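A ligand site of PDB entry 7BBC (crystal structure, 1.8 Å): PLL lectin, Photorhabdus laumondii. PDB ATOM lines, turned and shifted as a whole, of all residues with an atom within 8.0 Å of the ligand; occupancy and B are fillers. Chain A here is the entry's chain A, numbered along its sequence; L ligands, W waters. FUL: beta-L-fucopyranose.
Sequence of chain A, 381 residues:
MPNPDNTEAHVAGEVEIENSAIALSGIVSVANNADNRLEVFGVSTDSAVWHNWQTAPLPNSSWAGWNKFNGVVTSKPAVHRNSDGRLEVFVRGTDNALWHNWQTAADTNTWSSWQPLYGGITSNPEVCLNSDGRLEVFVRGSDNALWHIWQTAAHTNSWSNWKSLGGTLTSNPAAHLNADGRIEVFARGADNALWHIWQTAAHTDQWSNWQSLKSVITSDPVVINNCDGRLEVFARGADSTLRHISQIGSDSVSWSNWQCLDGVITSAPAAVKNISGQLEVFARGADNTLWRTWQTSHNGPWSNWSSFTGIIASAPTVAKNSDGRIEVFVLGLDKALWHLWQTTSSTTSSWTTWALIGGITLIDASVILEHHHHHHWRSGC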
ATOM      1  N   SER A  47      -5.575  16.458  28.658  1.00  0.00           N
ATOM      2  CA  SER A  47      -6.116  16.794  27.341  1.00  0.00           C
ATOM      3  C   SER A  47      -5.245  17.775  26.576  1.00  0.00           C
ATOM      4  O   SER A  47      -5.742  18.473  25.691  1.00  0.00           O
ATOM      5  CB  SER A  47      -7.536  17.323  27.453  1.00  0.00           C
ATOM      6  OG  SER A  47      -8.382  16.261  27.793  1.00  0.00           O
ATOM      7  N   VAL A  49      -1.545  18.303  24.302  1.00  0.00           N
ATOM      8  CA  VAL A  49      -0.536  17.599  23.496  1.00  0.00           C
ATOM      9  C   VAL A  49       0.818  17.697  24.164  1.00  0.00           C
ATOM     10  O   VAL A  49       1.292  18.788  24.502  1.00  0.00           O
ATOM     11  CB  VAL A  49      -0.460  18.183  22.077  1.00  0.00           C
ATOM     12  CG1 VAL A  49       0.700  17.543  21.265  1.00  0.00           C
ATOM     13  CG2 VAL A  49      -1.768  17.983  21.354  1.00  0.00           C
ATOM     14  N   PHE A  69       2.741  21.169  25.312  1.00  0.00           N
ATOM     15  CA  PHE A  69       2.204  22.337  24.666  1.00  0.00           C
ATOM     16  C   PHE A  69       0.979  22.816  25.457  1.00  0.00           C
ATOM     17  O   PHE A  69       0.041  22.045  25.666  1.00  0.00           O
ATOM     18  CB  PHE A  69       1.740  22.045  23.237  1.00  0.00           C
ATOM     19  CG  PHE A  69       2.828  21.647  22.251  1.00  0.00           C
ATOM     20  CD1 PHE A  69       4.058  22.274  22.236  1.00  0.00           C
ATOM     21  CD2 PHE A  69       2.563  20.704  21.280  1.00  0.00           C
ATOM     22  CE1 PHE A  69       4.997  21.937  21.299  1.00  0.00           C
ATOM     23  CE2 PHE A  69       3.510  20.353  20.371  1.00  0.00           C
ATOM     24  CZ  PHE A  69       4.719  20.962  20.374  1.00  0.00           C
ATOM     25  N   ASN A  70       0.925  24.078  25.805  1.00  0.00           N
ATOM     26  CA  ASN A  70      -0.244  24.550  26.551  1.00  0.00           C
ATOM     27  C   ASN A  70      -1.459  24.605  25.636  1.00  0.00           C
ATOM     28  O   ASN A  70      -1.348  25.015  24.487  1.00  0.00           O
ATOM     29  CB  ASN A  70       0.028  25.926  27.152  1.00  0.00           C
ATOM     30  CG  ASN A  70       0.922  25.848  28.388  1.00  0.00           C
ATOM     31  OD1 ASN A  70       0.798  24.932  29.205  1.00  0.00           O
ATOM     32  ND2 ASN A  70       1.830  26.793  28.512  1.00  0.00           N
ATOM     33  N   GLY A  71      -2.590  24.121  26.103  1.00  0.00           N
ATOM     34  CA  GLY A  71      -3.839  24.219  25.377  1.00  0.00           C
ATOM     35  C   GLY A  71      -4.565  22.883  25.383  1.00  0.00           C
ATOM     36  O   GLY A  71      -3.912  21.847  25.318  1.00  0.00           O
ATOM     37  N   VAL A  72      -5.875  22.906  25.512  1.00  0.00           N
ATOM     38  CA  VAL A  72      -6.700  21.717  25.540  1.00  0.00           C
ATOM     39  C   VAL A  72      -7.128  21.421  24.110  1.00  0.00           C
ATOM     40  O   VAL A  72      -7.520  22.319  23.361  1.00  0.00           O
ATOM     41  CB  VAL A  72      -7.918  21.923  26.468  1.00  0.00           C
ATOM     42  CG1 VAL A  72      -8.881  20.754  26.376  1.00  0.00           C
ATOM     43  CG2 VAL A  72      -7.424  22.103  27.891  1.00  0.00           C
ATOM     44  N   VAL A  73      -7.089  20.144  23.751  1.00  0.00           N
ATOM     45  CA  VAL A  73      -7.351  19.704  22.387  1.00  0.00           C
ATOM     46  C   VAL A  73      -8.417  18.636  22.432  1.00  0.00           C
ATOM     47  O   VAL A  73      -8.674  18.027  23.474  1.00  0.00           O
ATOM     48  CB  VAL A  73      -6.076  19.184  21.644  1.00  0.00           C
ATOM     49  CG1 VAL A  73      -4.993  20.212  21.674  1.00  0.00           C
ATOM     50  CG2 VAL A  73      -5.550  17.809  22.190  1.00  0.00           C
ATOM     51  N   THR A  74      -9.057  18.436  21.285  1.00  0.00           N
ATOM     52  CA  THR A  74     -10.155  17.502  21.185  1.00  0.00           C
ATOM     53  C   THR A  74     -10.029  16.546  20.014  1.00  0.00           C
ATOM     54  O   THR A  74     -11.042  16.006  19.561  1.00  0.00           O
ATOM     55  CB  THR A  74     -11.487  18.231  21.060  1.00  0.00           C
ATOM     56  OG1 THR A  74     -11.468  19.034  19.868  1.00  0.00           O
ATOM     57  CG2 THR A  74     -11.742  19.115  22.269  1.00  0.00           C
ATOM     58  N   VAL A  91      -4.438  20.109  15.081  1.00  0.00           N
ATOM     59  CA  VAL A  91      -5.287  19.456  16.081  1.00  0.00           C
ATOM     60  C   VAL A  91      -6.591  20.232  16.169  1.00  0.00           C
ATOM     61  O   VAL A  91      -6.633  21.442  15.926  1.00  0.00           O
ATOM     62  CB  VAL A  91      -4.554  19.399  17.448  1.00  0.00           C
ATOM     63  CG1 VAL A  91      -4.648  20.724  18.193  1.00  0.00           C
ATOM     64  CG2 VAL A  91      -5.081  18.304  18.290  1.00  0.00           C
ATOM     65  N   ARG A  92      -7.667  19.529  16.521  1.00  0.00           N
ATOM     66  CA  ARG A  92      -8.950  20.163  16.771  1.00  0.00           C
ATOM     67  C   ARG A  92      -8.923  20.770  18.173  1.00  0.00           C
ATOM     68  O   ARG A  92      -8.386  20.164  19.112  1.00  0.00           O
ATOM     69  CB  ARG A  92     -10.089  19.168  16.624  1.00  0.00           C
ATOM     70  CG  ARG A  92     -11.472  19.871  16.563  1.00  0.00           C
ATOM     71  CD  ARG A  92     -12.651  18.916  16.345  1.00  0.00           C
ATOM     72  NE  ARG A  92     -12.876  18.028  17.486  1.00  0.00           N
ATOM     73  CZ  ARG A  92     -13.904  17.218  17.615  1.00  0.00           C
ATOM     74  NH1 ARG A  92     -14.833  17.158  16.681  1.00  0.00           N
ATOM     75  NH2 ARG A  92     -13.993  16.450  18.686  1.00  0.00           N
ATOM     76  N   GLY A  93      -9.487  21.969  18.297  1.00  0.00           N
ATOM     77  CA  GLY A  93      -9.530  22.676  19.561  1.00  0.00           C
ATOM     78  C   GLY A  93     -10.864  22.505  20.281  1.00  0.00           C
ATOM     79  O   GLY A  93     -11.766  21.818  19.825  1.00  0.00           O
ATOM     80  N   THR A  94     -10.945  23.108  21.471  1.00  0.00           N
ATOM     81  CA  THR A  94     -12.180  23.082  22.260  1.00  0.00           C
ATOM     82  C   THR A  94     -13.351  23.740  21.546  1.00  0.00           C
ATOM     83  O   THR A  94     -14.495  23.439  21.898  1.00  0.00           O
ATOM     84  CB  THR A  94     -11.971  23.769  23.616  1.00  0.00           C
ATOM     85  OG1 THR A  94     -11.488  25.101  23.429  1.00  0.00           O
ATOM     86  CG2 THR A  94     -10.950  23.032  24.408  1.00  0.00           C
ATOM     87  N   ASP A  95     -13.087  24.585  20.570  1.00  0.00           N
ATOM     88  CA  ASP A  95     -14.117  25.234  19.774  1.00  0.00           C
ATOM     89  C   ASP A  95     -14.465  24.469  18.516  1.00  0.00           C
ATOM     90  O   ASP A  95     -15.209  24.982  17.676  1.00  0.00           O
ATOM     91  CB  ASP A  95     -13.695  26.636  19.398  1.00  0.00           C
ATOM     92  CG  ASP A  95     -12.323  26.700  18.724  1.00  0.00           C
ATOM     93  OD1 ASP A  95     -11.704  25.649  18.428  1.00  0.00           O
ATOM     94  OD2 ASP A  95     -11.858  27.826  18.483  1.00  0.00           O
ATOM     95  N   ASN A  96     -13.963  23.250  18.400  1.00  0.00           N
ATOM     96  CA  ASN A  96     -14.142  22.389  17.249  1.00  0.00           C
ATOM     97  C   ASN A  96     -13.541  22.939  15.973  1.00  0.00           C
ATOM     98  O   ASN A  96     -13.827  22.425  14.873  1.00  0.00           O
ATOM     99  CB  ASN A  96     -15.621  22.057  17.072  1.00  0.00           C
ATOM    100  CG  ASN A  96     -16.081  21.039  18.103  1.00  0.00           C
ATOM    101  OD1 ASN A  96     -15.304  20.223  18.575  1.00  0.00           O
ATOM    102  ND2 ASN A  96     -17.321  21.142  18.504  1.00  0.00           N
ATOM    103  N   ALA A  97     -12.663  23.921  16.099  1.00  0.00           N
ATOM    104  CA  ALA A  97     -11.954  24.450  14.951  1.00  0.00           C
ATOM    105  C   ALA A  97     -10.572  23.813  14.859  1.00  0.00           C
ATOM    106  O   ALA A  97     -10.106  23.118  15.770  1.00  0.00           O
ATOM    107  CB  ALA A  97     -11.848  25.969  15.043  1.00  0.00           C
ATOM    108  N   LEU A  98      -9.918  24.091  13.754  1.00  0.00           N
ATOM    109  CA  LEU A  98      -8.566  23.622  13.495  1.00  0.00           C
ATOM    110  C   LEU A  98      -7.535  24.608  14.020  1.00  0.00           C
ATOM    111  O   LEU A  98      -7.642  25.818  13.770  1.00  0.00           O
ATOM    112  CB  LEU A  98      -8.357  23.406  11.999  1.00  0.00           C
ATOM    113  CG  LEU A  98      -7.032  22.722  11.591  1.00  0.00           C
ATOM    114  CD1 LEU A  98      -7.021  21.307  12.025  1.00  0.00           C
ATOM    115  CD2 LEU A  98      -6.815  22.848  10.043  1.00  0.00           C
ATOM    116  N   TRP A  99      -6.558  24.088  14.753  1.00  0.00           N
ATOM    117  CA  TRP A  99      -5.446  24.859  15.283  1.00  0.00           C
ATOM    118  C   TRP A  99      -4.122  24.238  14.817  1.00  0.00           C
ATOM    119  O   TRP A  99      -4.060  23.039  14.500  1.00  0.00           O
ATOM    120  CB  TRP A  99      -5.496  24.896  16.804  1.00  0.00           C
ATOM    121  CG  TRP A  99      -6.717  25.674  17.314  1.00  0.00           C
ATOM    122  CD1 TRP A  99      -8.000  25.257  17.328  1.00  0.00           C
ATOM    123  CD2 TRP A  99      -6.719  26.990  17.877  1.00  0.00           C
ATOM    124  NE1 TRP A  99      -8.824  26.222  17.863  1.00  0.00           N
ATOM    125  CE2 TRP A  99      -8.057  27.308  18.188  1.00  0.00           C
ATOM    126  CE3 TRP A  99      -5.725  27.923  18.136  1.00  0.00           C
ATOM    127  CZ2 TRP A  99      -8.409  28.502  18.785  1.00  0.00           C
ATOM    128  CZ3 TRP A  99      -6.064  29.113  18.694  1.00  0.00           C
ATOM    129  CH2 TRP A  99      -7.402  29.403  19.016  1.00  0.00           C
ATOM    130  N   HIS A 100      -3.086  25.054  14.742  1.00  0.00           N
ATOM    131  CA  HIS A 100      -1.778  24.513  14.389  1.00  0.00           C
ATOM    132  C   HIS A 100      -0.669  25.216  15.144  1.00  0.00           C
ATOM    133  O   HIS A 100      -0.828  26.334  15.622  1.00  0.00           O
ATOM    134  CB  HIS A 100      -1.490  24.566  12.857  1.00  0.00           C
ATOM    135  CG  HIS A 100      -1.450  25.913  12.234  1.00  0.00           C
ATOM    136  ND1 HIS A 100      -0.548  26.232  11.232  1.00  0.00           N
ATOM    137  CD2 HIS A 100      -2.224  27.009  12.410  1.00  0.00           C
ATOM    138  CE1 HIS A 100      -0.735  27.486  10.847  1.00  0.00           C
ATOM    139  NE2 HIS A 100      -1.762  27.970  11.536  1.00  0.00           N
ATOM    140  N   SER A 113       3.295  28.069  19.445  1.00  0.00           N
ATOM    141  CA  SER A 113       2.076  27.981  20.240  1.00  0.00           C
ATOM    142  C   SER A 113       0.894  27.909  19.280  1.00  0.00           C
ATOM    143  O   SER A 113       1.054  28.109  18.067  1.00  0.00           O
ATOM    144  CB  SER A 113       1.907  29.144  21.235  1.00  0.00           C
ATOM    145  OG  SER A 113       1.446  30.340  20.604  1.00  0.00           O
ATOM    146  N   TRP A 114      -0.283  27.592  19.784  1.00  0.00           N
ATOM    147  CA  TRP A 114      -1.369  27.210  18.900  1.00  0.00           C
ATOM    148  C   TRP A 114      -1.957  28.452  18.252  1.00  0.00           C
ATOM    149  O   TRP A 114      -2.258  29.435  18.921  1.00  0.00           O
ATOM    150  CB  TRP A 114      -2.479  26.489  19.652  1.00  0.00           C
ATOM    151  CG  TRP A 114      -2.111  25.143  20.221  1.00  0.00           C
ATOM    152  CD1 TRP A 114      -1.985  24.818  21.547  1.00  0.00           C
ATOM    153  CD2 TRP A 114      -1.809  23.966  19.492  1.00  0.00           C
ATOM    154  NE1 TRP A 114      -1.658  23.528  21.684  1.00  0.00           N
ATOM    155  CE2 TRP A 114      -1.525  22.960  20.435  1.00  0.00           C
ATOM    156  CE3 TRP A 114      -1.761  23.638  18.145  1.00  0.00           C
ATOM    157  CZ2 TRP A 114      -1.184  21.669  20.078  1.00  0.00           C
ATOM    158  CZ3 TRP A 114      -1.434  22.350  17.785  1.00  0.00           C
ATOM    159  CH2 TRP A 114      -1.145  21.379  18.746  1.00  0.00           C
ATOM    160  N   GLN A 115      -2.178  28.389  16.959  1.00  0.00           N
ATOM    161  CA  GLN A 115      -2.739  29.494  16.197  1.00  0.00           C
ATOM    162  C   GLN A 115      -3.935  28.990  15.404  1.00  0.00           C
ATOM    163  O   GLN A 115      -3.967  27.830  14.987  1.00  0.00           O
ATOM    164  CB  GLN A 115      -1.711  30.063  15.208  1.00  0.00           C
ATOM    165  CG  GLN A 115      -0.399  30.471  15.830  1.00  0.00           C
ATOM    166  CD  GLN A 115      -0.482  31.591  16.777  1.00  0.00           C
ATOM    167  OE1 GLN A 115       0.262  31.650  17.778  1.00  0.00           O
ATOM    168  NE2 GLN A 115      -1.353  32.514  16.494  1.00  0.00           N
ATOM    169  N   PRO A 116      -4.920  29.847  15.167  1.00  0.00           N
ATOM    170  CA  PRO A 116      -6.187  29.357  14.629  1.00  0.00           C
ATOM    171  C   PRO A 116      -6.210  29.281  13.112  1.00  0.00           C
ATOM    172  O   PRO A 116      -5.770  30.198  12.420  1.00  0.00           O
ATOM    173  CB  PRO A 116      -7.200  30.422  15.101  1.00  0.00           C
ATOM    174  CG  PRO A 116      -6.410  31.651  15.204  1.00  0.00           C
ATOM    175  CD  PRO A 116      -5.045  31.224  15.705  1.00  0.00           C
HETATM  176  C1  FUL L   1      -6.385  26.970  23.367  1.00  0.00           C
HETATM  177  C2  FUL L   1      -7.910  26.955  23.466  1.00  0.00           C
HETATM  178  O2  FUL L   1      -8.425  28.138  24.122  1.00  0.00           O
HETATM  179  C3  FUL L   1      -8.412  26.822  22.063  1.00  0.00           C
HETATM  180  O3  FUL L   1      -9.866  26.752  22.009  1.00  0.00           O
HETATM  181  C4  FUL L   1      -7.883  25.567  21.368  1.00  0.00           C
HETATM  182  O4  FUL L   1      -8.469  24.416  22.000  1.00  0.00           O
HETATM  183  C5  FUL L   1      -6.358  25.488  21.432  1.00  0.00           C
HETATM  184  C6  FUL L   1      -5.779  24.169  21.007  1.00  0.00           C
HETATM  185  O5  FUL L   1      -5.916  25.664  22.809  1.00  0.00           O
HETATM  186  O1  FUL L   1      -5.809  27.119  24.586  1.00  0.00           O
HETATM  187  O   HOH W   1      -6.976  25.731  26.225  1.00  0.00           O
HETATM  188  O   HOH W   2     -11.058  29.130  21.421  1.00  0.00           O
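The backbone NH (N) of Trp 99 is in hydrogen-bond range of the backbone carbonyl oxygen (O) of Val 91 (2.9 Å). OG1 of Thr 74 sits at hydrogen-bond distance from O of Gly 93 (2.8 Å). The indole nitrogen (NE1) of Trp 99 is in hydrogen-bond range of the side-chain carboxylate (OD1) of Asp 95, at 3.0 Å. NE1 of Trp 114 lies close to O of Asn 70.
Merely in contact with the ligand: Gly 93 (3.2 Å), Gly 71 (3.6 Å), Trp 99 (3.6 Å) and Trp 114 (3.9 Å). Six residues have an atom within 4 Å of the ligand: Gly 71, Val 72, Gly 93, Thr 94, Trp 99 and Trp 114.
OG1 of Thr 94 sits at hydrogen-bond distance from O3 of the ligand. An oxygen (O4) of the ligand is in hydrogen-bond range of the backbone NH (N) of Thr 94, at 2.8 Å. The backbone carbonyl oxygen of Val 72 sits at hydrogen-bond distance from an oxygen (O4) of the ligand (2.7 Å).
Water W1 bridges O1 of the ligand (2.4 Å) and N of Val 72 (3.1 Å). Water W2 lies within hydrogen-bond range of an oxygen (O3) of the ligand (2.7 Å) and the side-chain carboxylate of Asp 95 (3.3 Å).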
